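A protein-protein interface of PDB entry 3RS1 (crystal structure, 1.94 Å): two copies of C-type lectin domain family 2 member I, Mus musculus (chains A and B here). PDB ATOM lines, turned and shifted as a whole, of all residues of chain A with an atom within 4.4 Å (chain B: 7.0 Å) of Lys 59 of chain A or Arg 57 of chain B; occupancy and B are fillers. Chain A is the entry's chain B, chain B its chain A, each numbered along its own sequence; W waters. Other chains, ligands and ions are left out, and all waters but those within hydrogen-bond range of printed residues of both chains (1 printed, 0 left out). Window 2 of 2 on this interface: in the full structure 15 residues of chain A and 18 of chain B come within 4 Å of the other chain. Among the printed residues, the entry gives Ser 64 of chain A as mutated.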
ATOM      1  N   PHE A  22       6.803  -8.974  -6.353  1.00  0.00           N
ATOM      2  CA  PHE A  22       7.873  -8.989  -5.374  1.00  0.00           C
ATOM      3  C   PHE A  22       8.986  -8.111  -5.907  1.00  0.00           C
ATOM      4  O   PHE A  22       9.452  -8.284  -7.047  1.00  0.00           O
ATOM      5  CB  PHE A  22       8.347 -10.427  -5.133  1.00  0.00           C
ATOM      6  CG  PHE A  22       7.311 -11.276  -4.463  1.00  0.00           C
ATOM      7  CD1 PHE A  22       7.341 -11.481  -3.104  1.00  0.00           C
ATOM      8  CD2 PHE A  22       6.229 -11.774  -5.187  1.00  0.00           C
ATOM      9  CE1 PHE A  22       6.354 -12.230  -2.475  1.00  0.00           C
ATOM     10  CE2 PHE A  22       5.279 -12.523  -4.582  1.00  0.00           C
ATOM     11  CZ  PHE A  22       5.312 -12.759  -3.235  1.00  0.00           C
ATOM     12  N   LEU A  55       2.885 -15.660   0.260  1.00  0.00           N
ATOM     13  CA  LEU A  55       3.706 -14.461   0.466  1.00  0.00           C
ATOM     14  C   LEU A  55       4.930 -14.776   1.295  1.00  0.00           C
ATOM     15  O   LEU A  55       6.021 -14.386   0.912  1.00  0.00           O
ATOM     16  CB  LEU A  55       2.925 -13.329   1.129  1.00  0.00           C
ATOM     17  CG  LEU A  55       1.747 -12.754   0.340  1.00  0.00           C
ATOM     18  CD1 LEU A  55       1.136 -11.553   1.054  1.00  0.00           C
ATOM     19  CD2 LEU A  55       2.178 -12.398  -1.105  1.00  0.00           C
ATOM     20  N   LYS A  56       4.762 -15.524   2.387  1.00  0.00           N
ATOM     21  CA  LYS A  56       5.905 -15.882   3.233  1.00  0.00           C
ATOM     22  C   LYS A  56       6.930 -16.789   2.535  1.00  0.00           C
ATOM     23  O   LYS A  56       8.157 -16.603   2.709  1.00  0.00           O
ATOM     24  CB  LYS A  56       5.454 -16.518   4.548  1.00  0.00           C
ATOM     25  CG  LYS A  56       4.721 -15.595   5.546  1.00  0.00           C
ATOM     26  CD  LYS A  56       4.133 -16.477   6.670  1.00  0.00           C
ATOM     27  CE  LYS A  56       3.450 -15.700   7.765  1.00  0.00           C
ATOM     28  NZ  LYS A  56       2.979 -16.589   8.902  1.00  0.00           N
ATOM     29  N   ARG A  57       6.458 -17.762   1.756  1.00  0.00           N
ATOM     30  CA  ARG A  57       7.365 -18.697   1.072  1.00  0.00           C
ATOM     31  C   ARG A  57       8.133 -17.990  -0.047  1.00  0.00           C
ATOM     32  O   ARG A  57       9.360 -18.147  -0.207  1.00  0.00           O
ATOM     33  CB  ARG A  57       6.600 -19.897   0.488  1.00  0.00           C
ATOM     34  CG  ARG A  57       6.001 -20.855   1.528  1.00  0.00           C
ATOM     35  CD  ARG A  57       5.652 -22.250   0.975  1.00  0.00           C
ATOM     36  NE  ARG A  57       6.854 -22.898   0.470  1.00  0.00           N
ATOM     37  CZ  ARG A  57       7.195 -23.025  -0.818  1.00  0.00           C
ATOM     38  NH1 ARG A  57       6.386 -22.632  -1.798  1.00  0.00           N
ATOM     39  NH2 ARG A  57       8.363 -23.579  -1.120  1.00  0.00           N
ATOM     40  N   PHE A  58       7.395 -17.214  -0.828  1.00  0.00           N
ATOM     41  CA  PHE A  58       7.939 -16.610  -2.003  1.00  0.00           C
ATOM     42  C   PHE A  58       8.901 -15.444  -1.700  1.00  0.00           C
ATOM     43  O   PHE A  58       9.914 -15.299  -2.388  1.00  0.00           O
ATOM     44  CB  PHE A  58       6.824 -16.160  -2.917  1.00  0.00           C
ATOM     45  CG  PHE A  58       7.199 -16.220  -4.380  1.00  0.00           C
ATOM     46  CD1 PHE A  58       7.321 -17.440  -5.013  1.00  0.00           C
ATOM     47  CD2 PHE A  58       7.473 -15.061  -5.086  1.00  0.00           C
ATOM     48  CE1 PHE A  58       7.675 -17.512  -6.348  1.00  0.00           C
ATOM     49  CE2 PHE A  58       7.832 -15.118  -6.428  1.00  0.00           C
ATOM     50  CZ  PHE A  58       7.933 -16.344  -7.057  1.00  0.00           C
ATOM     51  N   LYS A  59       8.612 -14.638  -0.677  1.00  0.00           N
ATOM     52  CA  LYS A  59       9.574 -13.589  -0.276  1.00  0.00           C
ATOM     53  C   LYS A  59      10.886 -14.182   0.265  1.00  0.00           C
ATOM     54  O   LYS A  59      11.927 -13.528   0.181  1.00  0.00           O
ATOM     55  CB  LYS A  59       8.987 -12.595   0.742  1.00  0.00           C
ATOM     56  CG  LYS A  59       8.631 -13.173   2.091  1.00  0.00           C
ATOM     57  CD  LYS A  59       9.732 -12.927   3.115  1.00  0.00           C
ATOM     58  CE  LYS A  59       9.505 -13.713   4.374  1.00  0.00           C
ATOM     59  NZ  LYS A  59       9.809 -15.161   4.197  1.00  0.00           N
ATOM     60  N   GLY A  60      10.820 -15.380   0.855  1.00  0.00           N
ATOM     61  CA  GLY A  60      12.025 -16.142   1.238  1.00  0.00           C
ATOM     62  C   GLY A  60      12.888 -15.475   2.295  1.00  0.00           C
ATOM     63  O   GLY A  60      12.395 -15.105   3.384  1.00  0.00           O
ATOM     64  N   ASP A  61      14.169 -15.314   1.962  1.00  0.00           N
ATOM     65  CA  ASP A  61      15.180 -14.763   2.863  1.00  0.00           C
ATOM     66  C   ASP A  61      15.133 -13.246   2.905  1.00  0.00           C
ATOM     67  O   ASP A  61      15.840 -12.633   3.695  1.00  0.00           O
ATOM     68  CB  ASP A  61      16.597 -15.190   2.426  1.00  0.00           C
ATOM     69  CG  ASP A  61      16.863 -16.670   2.615  1.00  0.00           C
ATOM     70  OD1 ASP A  61      16.319 -17.254   3.567  1.00  0.00           O
ATOM     71  OD2 ASP A  61      17.619 -17.258   1.800  1.00  0.00           O
ATOM     72  N   PHE A  62      14.295 -12.640   2.064  1.00  0.00           N
ATOM     73  CA  PHE A  62      14.188 -11.177   2.001  1.00  0.00           C
ATOM     74  C   PHE A  62      13.033 -10.657   2.855  1.00  0.00           C
ATOM     75  O   PHE A  62      11.880 -10.839   2.494  1.00  0.00           O
ATOM     76  CB  PHE A  62      13.975 -10.748   0.547  1.00  0.00           C
ATOM     77  CG  PHE A  62      15.153 -11.041  -0.357  1.00  0.00           C
ATOM     78  CD1 PHE A  62      16.305 -10.260  -0.304  1.00  0.00           C
ATOM     79  CD2 PHE A  62      15.096 -12.083  -1.274  1.00  0.00           C
ATOM     80  CE1 PHE A  62      17.393 -10.538  -1.135  1.00  0.00           C
ATOM     81  CE2 PHE A  62      16.177 -12.361  -2.111  1.00  0.00           C
ATOM     82  CZ  PHE A  62      17.330 -11.578  -2.033  1.00  0.00           C
ATOM     83  N   SER A  64      10.196  -8.493   3.983  1.00  0.00           N
ATOM     84  CA  SER A  64       9.381  -7.795   3.003  1.00  0.00           C
ATOM     85  C   SER A  64       8.237  -7.032   3.588  1.00  0.00           C
ATOM     86  O   SER A  64       7.397  -7.574   4.342  1.00  0.00           O
ATOM     87  CB  SER A  64       8.877  -8.775   1.943  1.00  0.00           C
ATOM     88  OG  SER A  64      10.020  -9.300   1.264  1.00  0.00           O
ATOM     89  N   LEU A 100       7.054  -9.061   6.518  1.00  0.00           N
ATOM     90  CA  LEU A 100       7.202 -10.501   6.659  1.00  0.00           C
ATOM     91  C   LEU A 100       8.667 -10.868   6.815  1.00  0.00           C
ATOM     92  O   LEU A 100       9.527 -10.362   6.082  1.00  0.00           O
ATOM     93  CB  LEU A 100       6.600 -11.238   5.451  1.00  0.00           C
ATOM     94  CG  LEU A 100       5.136 -10.913   5.175  1.00  0.00           C
ATOM     95  CD1 LEU A 100       4.703 -11.461   3.804  1.00  0.00           C
ATOM     96  CD2 LEU A 100       4.260 -11.473   6.333  1.00  0.00           C
ATOM     97  N   SER A 101       8.926 -11.764   7.754  1.00  0.00           N
ATOM     98  CA  SER A 101      10.249 -12.216   8.070  1.00  0.00           C
ATOM     99  C   SER A 101      10.201 -13.704   8.388  1.00  0.00           C
ATOM    100  O   SER A 101       9.444 -14.112   9.267  1.00  0.00           O
ATOM    101  CB  SER A 101      10.773 -11.456   9.275  1.00  0.00           C
ATOM    102  OG  SER A 101      12.157 -11.643   9.332  1.00  0.00           O
ATOM    103  N   SER A 102      11.013 -14.496   7.680  1.00  0.00           N
ATOM    104  CA  SER A 102      10.927 -15.965   7.696  1.00  0.00           C
ATOM    105  C   SER A 102       9.462 -16.364   7.596  1.00  0.00           C
ATOM    106  O   SER A 102       8.846 -16.087   6.574  1.00  0.00           O
ATOM    107  CB  SER A 102      11.640 -16.562   8.932  1.00  0.00           C
ATOM    108  OG  SER A 102      10.969 -16.245  10.141  1.00  0.00           O
ATOM    109  N   LEU B  52      10.348 -20.271 -15.442  1.00  0.00           N
ATOM    110  CA  LEU B  52      11.547 -20.824 -14.815  1.00  0.00           C
ATOM    111  C   LEU B  52      12.004 -20.036 -13.580  1.00  0.00           C
ATOM    112  O   LEU B  52      12.372 -20.633 -12.541  1.00  0.00           O
ATOM    113  CB  LEU B  52      12.696 -20.921 -15.832  1.00  0.00           C
ATOM    114  CG  LEU B  52      13.918 -21.662 -15.309  1.00  0.00           C
ATOM    115  CD1 LEU B  52      13.518 -23.092 -14.943  1.00  0.00           C
ATOM    116  CD2 LEU B  52      15.115 -21.676 -16.311  1.00  0.00           C
ATOM    117  N   ILE B  53      11.997 -18.710 -13.687  1.00  0.00           N
ATOM    118  CA  ILE B  53      12.387 -17.833 -12.572  1.00  0.00           C
ATOM    119  C   ILE B  53      11.426 -18.041 -11.390  1.00  0.00           C
ATOM    120  O   ILE B  53      11.845 -18.127 -10.219  1.00  0.00           O
ATOM    121  CB  ILE B  53      12.432 -16.340 -12.994  1.00  0.00           C
ATOM    122  CG1 ILE B  53      13.553 -16.097 -14.010  1.00  0.00           C
ATOM    123  CG2 ILE B  53      12.634 -15.424 -11.756  1.00  0.00           C
ATOM    124  CD1 ILE B  53      13.501 -14.683 -14.600  1.00  0.00           C
ATOM    125  N   PHE B  54      10.142 -18.170 -11.701  1.00  0.00           N
ATOM    126  CA  PHE B  54       9.158 -18.504 -10.681  1.00  0.00           C
ATOM    127  C   PHE B  54       9.480 -19.847 -10.017  1.00  0.00           C
ATOM    128  O   PHE B  54       9.495 -19.925  -8.783  1.00  0.00           O
ATOM    129  CB  PHE B  54       7.728 -18.467 -11.227  1.00  0.00           C
ATOM    130  CG  PHE B  54       6.722 -19.118 -10.319  1.00  0.00           C
ATOM    131  CD1 PHE B  54       6.150 -18.422  -9.296  1.00  0.00           C
ATOM    132  CD2 PHE B  54       6.373 -20.440 -10.502  1.00  0.00           C
ATOM    133  CE1 PHE B  54       5.242 -19.030  -8.436  1.00  0.00           C
ATOM    134  CE2 PHE B  54       5.459 -21.056  -9.646  1.00  0.00           C
ATOM    135  CZ  PHE B  54       4.900 -20.347  -8.628  1.00  0.00           C
ATOM    136  N   LEU B  55       9.764 -20.895 -10.799  1.00  0.00           N
ATOM    137  CA  LEU B  55      10.033 -22.208 -10.187  1.00  0.00           C
ATOM    138  C   LEU B  55      11.283 -22.156  -9.307  1.00  0.00           C
ATOM    139  O   LEU B  55      11.298 -22.730  -8.210  1.00  0.00           O
ATOM    140  CB  LEU B  55      10.148 -23.329 -11.229  1.00  0.00           C
ATOM    141  CG  LEU B  55       8.917 -23.578 -12.121  1.00  0.00           C
ATOM    142  CD1 LEU B  55       9.273 -24.466 -13.343  1.00  0.00           C
ATOM    143  CD2 LEU B  55       7.743 -24.185 -11.347  1.00  0.00           C
ATOM    144  N   LYS B  56      12.313 -21.446  -9.754  1.00  0.00           N
ATOM    145  CA  LYS B  56      13.566 -21.403  -8.997  1.00  0.00           C
ATOM    146  C   LYS B  56      13.344 -20.713  -7.643  1.00  0.00           C
ATOM    147  O   LYS B  56      13.946 -21.119  -6.658  1.00  0.00           O
ATOM    148  CB  LYS B  56      14.687 -20.755  -9.806  1.00  0.00           C
ATOM    149  CG  LYS B  56      15.141 -21.648 -10.975  1.00  0.00           C
ATOM    150  CD  LYS B  56      16.050 -20.885 -11.935  1.00  0.00           C
ATOM    151  CE  LYS B  56      16.793 -21.813 -12.866  1.00  0.00           C
ATOM    152  NZ  LYS B  56      17.618 -20.978 -13.799  1.00  0.00           N
ATOM    153  N   ARG B  57      12.408 -19.752  -7.593  1.00  0.00           N
ATOM    154  CA  ARG B  57      11.982 -19.149  -6.333  1.00  0.00           C
ATOM    155  C   ARG B  57      10.949 -19.942  -5.470  1.00  0.00           C
ATOM    156  O   ARG B  57      11.086 -20.022  -4.241  1.00  0.00           O
ATOM    157  CB  ARG B  57      11.417 -17.771  -6.632  1.00  0.00           C
ATOM    158  CG  ARG B  57      11.303 -16.892  -5.413  1.00  0.00           C
ATOM    159  CD  ARG B  57      11.368 -15.449  -5.830  1.00  0.00           C
ATOM    160  NE  ARG B  57      11.278 -14.563  -4.687  1.00  0.00           N
ATOM    161  CZ  ARG B  57      11.392 -13.239  -4.746  1.00  0.00           C
ATOM    162  NH1 ARG B  57      11.641 -12.631  -5.904  1.00  0.00           N
ATOM    163  NH2 ARG B  57      11.268 -12.528  -3.631  1.00  0.00           N
ATOM    164  N   PHE B  58       9.937 -20.519  -6.116  1.00  0.00           N
ATOM    165  CA  PHE B  58       8.843 -21.273  -5.469  1.00  0.00           C
ATOM    166  C   PHE B  58       9.341 -22.501  -4.672  1.00  0.00           C
ATOM    167  O   PHE B  58       8.720 -22.907  -3.676  1.00  0.00           O
ATOM    168  CB  PHE B  58       7.858 -21.686  -6.592  1.00  0.00           C
ATOM    169  CG  PHE B  58       6.526 -22.237  -6.142  1.00  0.00           C
ATOM    170  CD1 PHE B  58       5.704 -21.533  -5.266  1.00  0.00           C
ATOM    171  CD2 PHE B  58       6.037 -23.408  -6.719  1.00  0.00           C
ATOM    172  CE1 PHE B  58       4.449 -22.044  -4.886  1.00  0.00           C
ATOM    173  CE2 PHE B  58       4.795 -23.929  -6.359  1.00  0.00           C
ATOM    174  CZ  PHE B  58       3.988 -23.239  -5.447  1.00  0.00           C
ATOM    175  N   LYS B  59      10.462 -23.088  -5.090  1.00  0.00           N
ATOM    176  CA  LYS B  59      11.051 -24.228  -4.392  1.00  0.00           C
ATOM    177  C   LYS B  59      11.721 -23.829  -3.056  1.00  0.00           C
ATOM    178  O   LYS B  59      12.059 -24.690  -2.270  1.00  0.00           O
ATOM    179  CB  LYS B  59      12.047 -24.962  -5.317  1.00  0.00           C
ATOM    180  CG  LYS B  59      13.345 -24.223  -5.545  1.00  0.00           C
ATOM    181  CD  LYS B  59      14.249 -24.898  -6.578  1.00  0.00           C
ATOM    182  CE  LYS B  59      15.710 -24.432  -6.461  1.00  0.00           C
ATOM    183  NZ  LYS B  59      15.922 -22.923  -6.385  1.00  0.00           N
ATOM    184  N   GLY B  60      11.917 -22.531  -2.801  1.00  0.00           N
ATOM    185  CA  GLY B  60      12.469 -22.072  -1.521  1.00  0.00           C
ATOM    186  C   GLY B  60      13.935 -22.472  -1.428  1.00  0.00           C
ATOM    187  O   GLY B  60      14.660 -22.321  -2.384  1.00  0.00           O
ATOM    188  N   ASP B  61      14.365 -23.024  -0.302  1.00  0.00           N
ATOM    189  CA  ASP B  61      15.771 -23.468  -0.170  1.00  0.00           C
ATOM    190  C   ASP B  61      15.958 -24.941  -0.554  1.00  0.00           C
ATOM    191  O   ASP B  61      17.071 -25.455  -0.483  1.00  0.00           O
ATOM    192  CB  ASP B  61      16.288 -23.240   1.260  1.00  0.00           C
ATOM    193  CG  ASP B  61      16.505 -21.792   1.565  1.00  0.00           C
ATOM    194  OD1 ASP B  61      17.262 -21.146   0.793  1.00  0.00           O
ATOM    195  OD2 ASP B  61      15.930 -21.294   2.565  1.00  0.00           O
ATOM    196  N   LEU B 100      15.716 -28.708 -10.163  1.00  0.00           N
ATOM    197  CA  LEU B 100      16.216 -27.350  -9.907  1.00  0.00           C
ATOM    198  C   LEU B 100      17.035 -27.363  -8.644  1.00  0.00           C
ATOM    199  O   LEU B 100      16.614 -27.938  -7.626  1.00  0.00           O
ATOM    200  CB  LEU B 100      15.055 -26.363  -9.756  1.00  0.00           C
ATOM    201  CG  LEU B 100      14.102 -26.286 -10.947  1.00  0.00           C
ATOM    202  CD1 LEU B 100      12.882 -25.350 -10.676  1.00  0.00           C
ATOM    203  CD2 LEU B 100      14.862 -25.869 -12.204  1.00  0.00           C
ATOM    204  N   SER B 102      19.429 -24.381  -6.406  1.00  0.00           N
ATOM    205  CA  SER B 102      19.782 -22.952  -6.387  1.00  0.00           C
ATOM    206  C   SER B 102      19.179 -22.292  -7.644  1.00  0.00           C
ATOM    207  O   SER B 102      17.983 -22.350  -7.839  1.00  0.00           O
ATOM    208  CB  SER B 102      21.308 -22.732  -6.297  1.00  0.00           C
ATOM    209  OG  SER B 102      21.764 -22.917  -4.967  1.00  0.00           O
ATOM    210  N   ILE B 117       7.631 -29.986  -7.687  1.00  0.00           N
ATOM    211  CA  ILE B 117       6.603 -29.063  -8.087  1.00  0.00           C
ATOM    212  C   ILE B 117       5.826 -29.688  -9.222  1.00  0.00           C
ATOM    213  O   ILE B 117       6.407 -30.250 -10.132  1.00  0.00           O
ATOM    214  CB  ILE B 117       7.215 -27.695  -8.520  1.00  0.00           C
ATOM    215  CG1 ILE B 117       7.971 -27.057  -7.340  1.00  0.00           C
ATOM    216  CG2 ILE B 117       6.104 -26.742  -9.059  1.00  0.00           C
ATOM    217  CD1 ILE B 117       8.837 -25.835  -7.698  1.00  0.00           C
HETATM  218  O   HOH W   1      11.740 -18.310  -1.912  1.00  0.00           O
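The backbone carbonyl oxygen of Lys 56 of chain A lies within hydrogen-bond range of the side-chain amino group of Lys 59 of chain A.
The side-chain amino group of Lys 59 of chain A lies within hydrogen-bond range of the backbone carbonyl oxygen of Ser 102 of chain A (2.7 Å).
O of Lys 56 of chain B sits at hydrogen-bond distance from NZ of Lys 59 of chain B, at 2.7 Å.
The side-chain amino group of Lys 59 of chain B sits at hydrogen-bond distance from the backbone carbonyl oxygen of Ser 102 of chain B, 2.6 Å away.
Of the 13 printed residues of chain B, 4 touch a printed residue of chain A.
Printed residues of chain B that touch a printed residue of chain A: Phe 54, Arg 57, Phe 58 and Lys 59.
Hydrophobic or aromatic side chains of chain B within 4 Å of the printed part of chain A: Phe 54 and Phe 58.
Printed residues of chain A that touch a printed residue of chain B: Phe 22, Arg 57, Phe 58 and Lys 59.
Hydrophobic or aromatic side chains of chain A that line the printed part of chain B: Phe 22 and Phe 58.
Among the printed residues, no Asp or Glu carboxylate lies within 4 Å of a Lys or Arg side-chain nitrogen of the other chain.
The guanidinium group (NH2) of Arg 57 of chain A sits at hydrogen-bond distance from the backbone carbonyl oxygen (O) of Phe 58 of chain B, 2.7 Å away.
The guanidinium group (NE) of Arg 57 of chain B lies within hydrogen-bond range of the backbone carbonyl oxygen (O) of Phe 58 of chain A (2.8 Å).
Water W1 lies within hydrogen-bond range of the backbone carbonyl oxygen (O) of Arg 57 of chain A (2.9 Å) and the backbone carbonyl oxygen (O) of Arg 57 of chain B (3.0 Å).
Among the printed residues, merely in contact across the chains: Phe 22 of chain A with Arg 57 of chain B, Arg 57 of chain A with Lys 59 of chain B, Phe 58 of chain A with Phe 54 of chain B, Phe 58 of chain A with Phe 58 of chain B and Lys 59 of chain A with Arg 57 of chain B.
Arg 57 of chain A touches Phe 58 of chain B, and with the chains exchanged Phe 58 of chain A touches Arg 57 of chain B.
Arg 57 of chain A touches Lys 59 of chain B, and with the chains exchanged Lys 59 of chain A touches Arg 57 of chain B.
Phe 58 of chain B touches its own counterpart, Phe 58 of chain A.
Printed residues of chain B within 4 Å of Phe 22 of chain A: Arg 57.
Printed residues of chain B within 4 Å of Arg 57 of chain A: Phe 58 and Lys 59.
Lys 59 of chain A touches one residue of chain B.
Of the printed residues of chain A, Phe 54 of chain B touches Phe 58.
Of chain A, only Phe 22 (3.9 Å), Phe 58 (2.8 Å) and Lys 59 (3.9 Å) come within 4 Å of Arg 57 of chain B.
Of the printed residues of chain A, Phe 58 of chain B touches Arg 57 and Phe 58.
Printed residues of chain A within 4 Å of Lys 59 of chain B: Arg 57.
The nearest printed residue of chain B that does not touch Lys 59 of chain A is Phe 58 of chain B (8.1 Å).
The nearest printed residue of chain B that does not touch Arg 57 of chain A is Gly 60 of chain B (4.1 Å).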
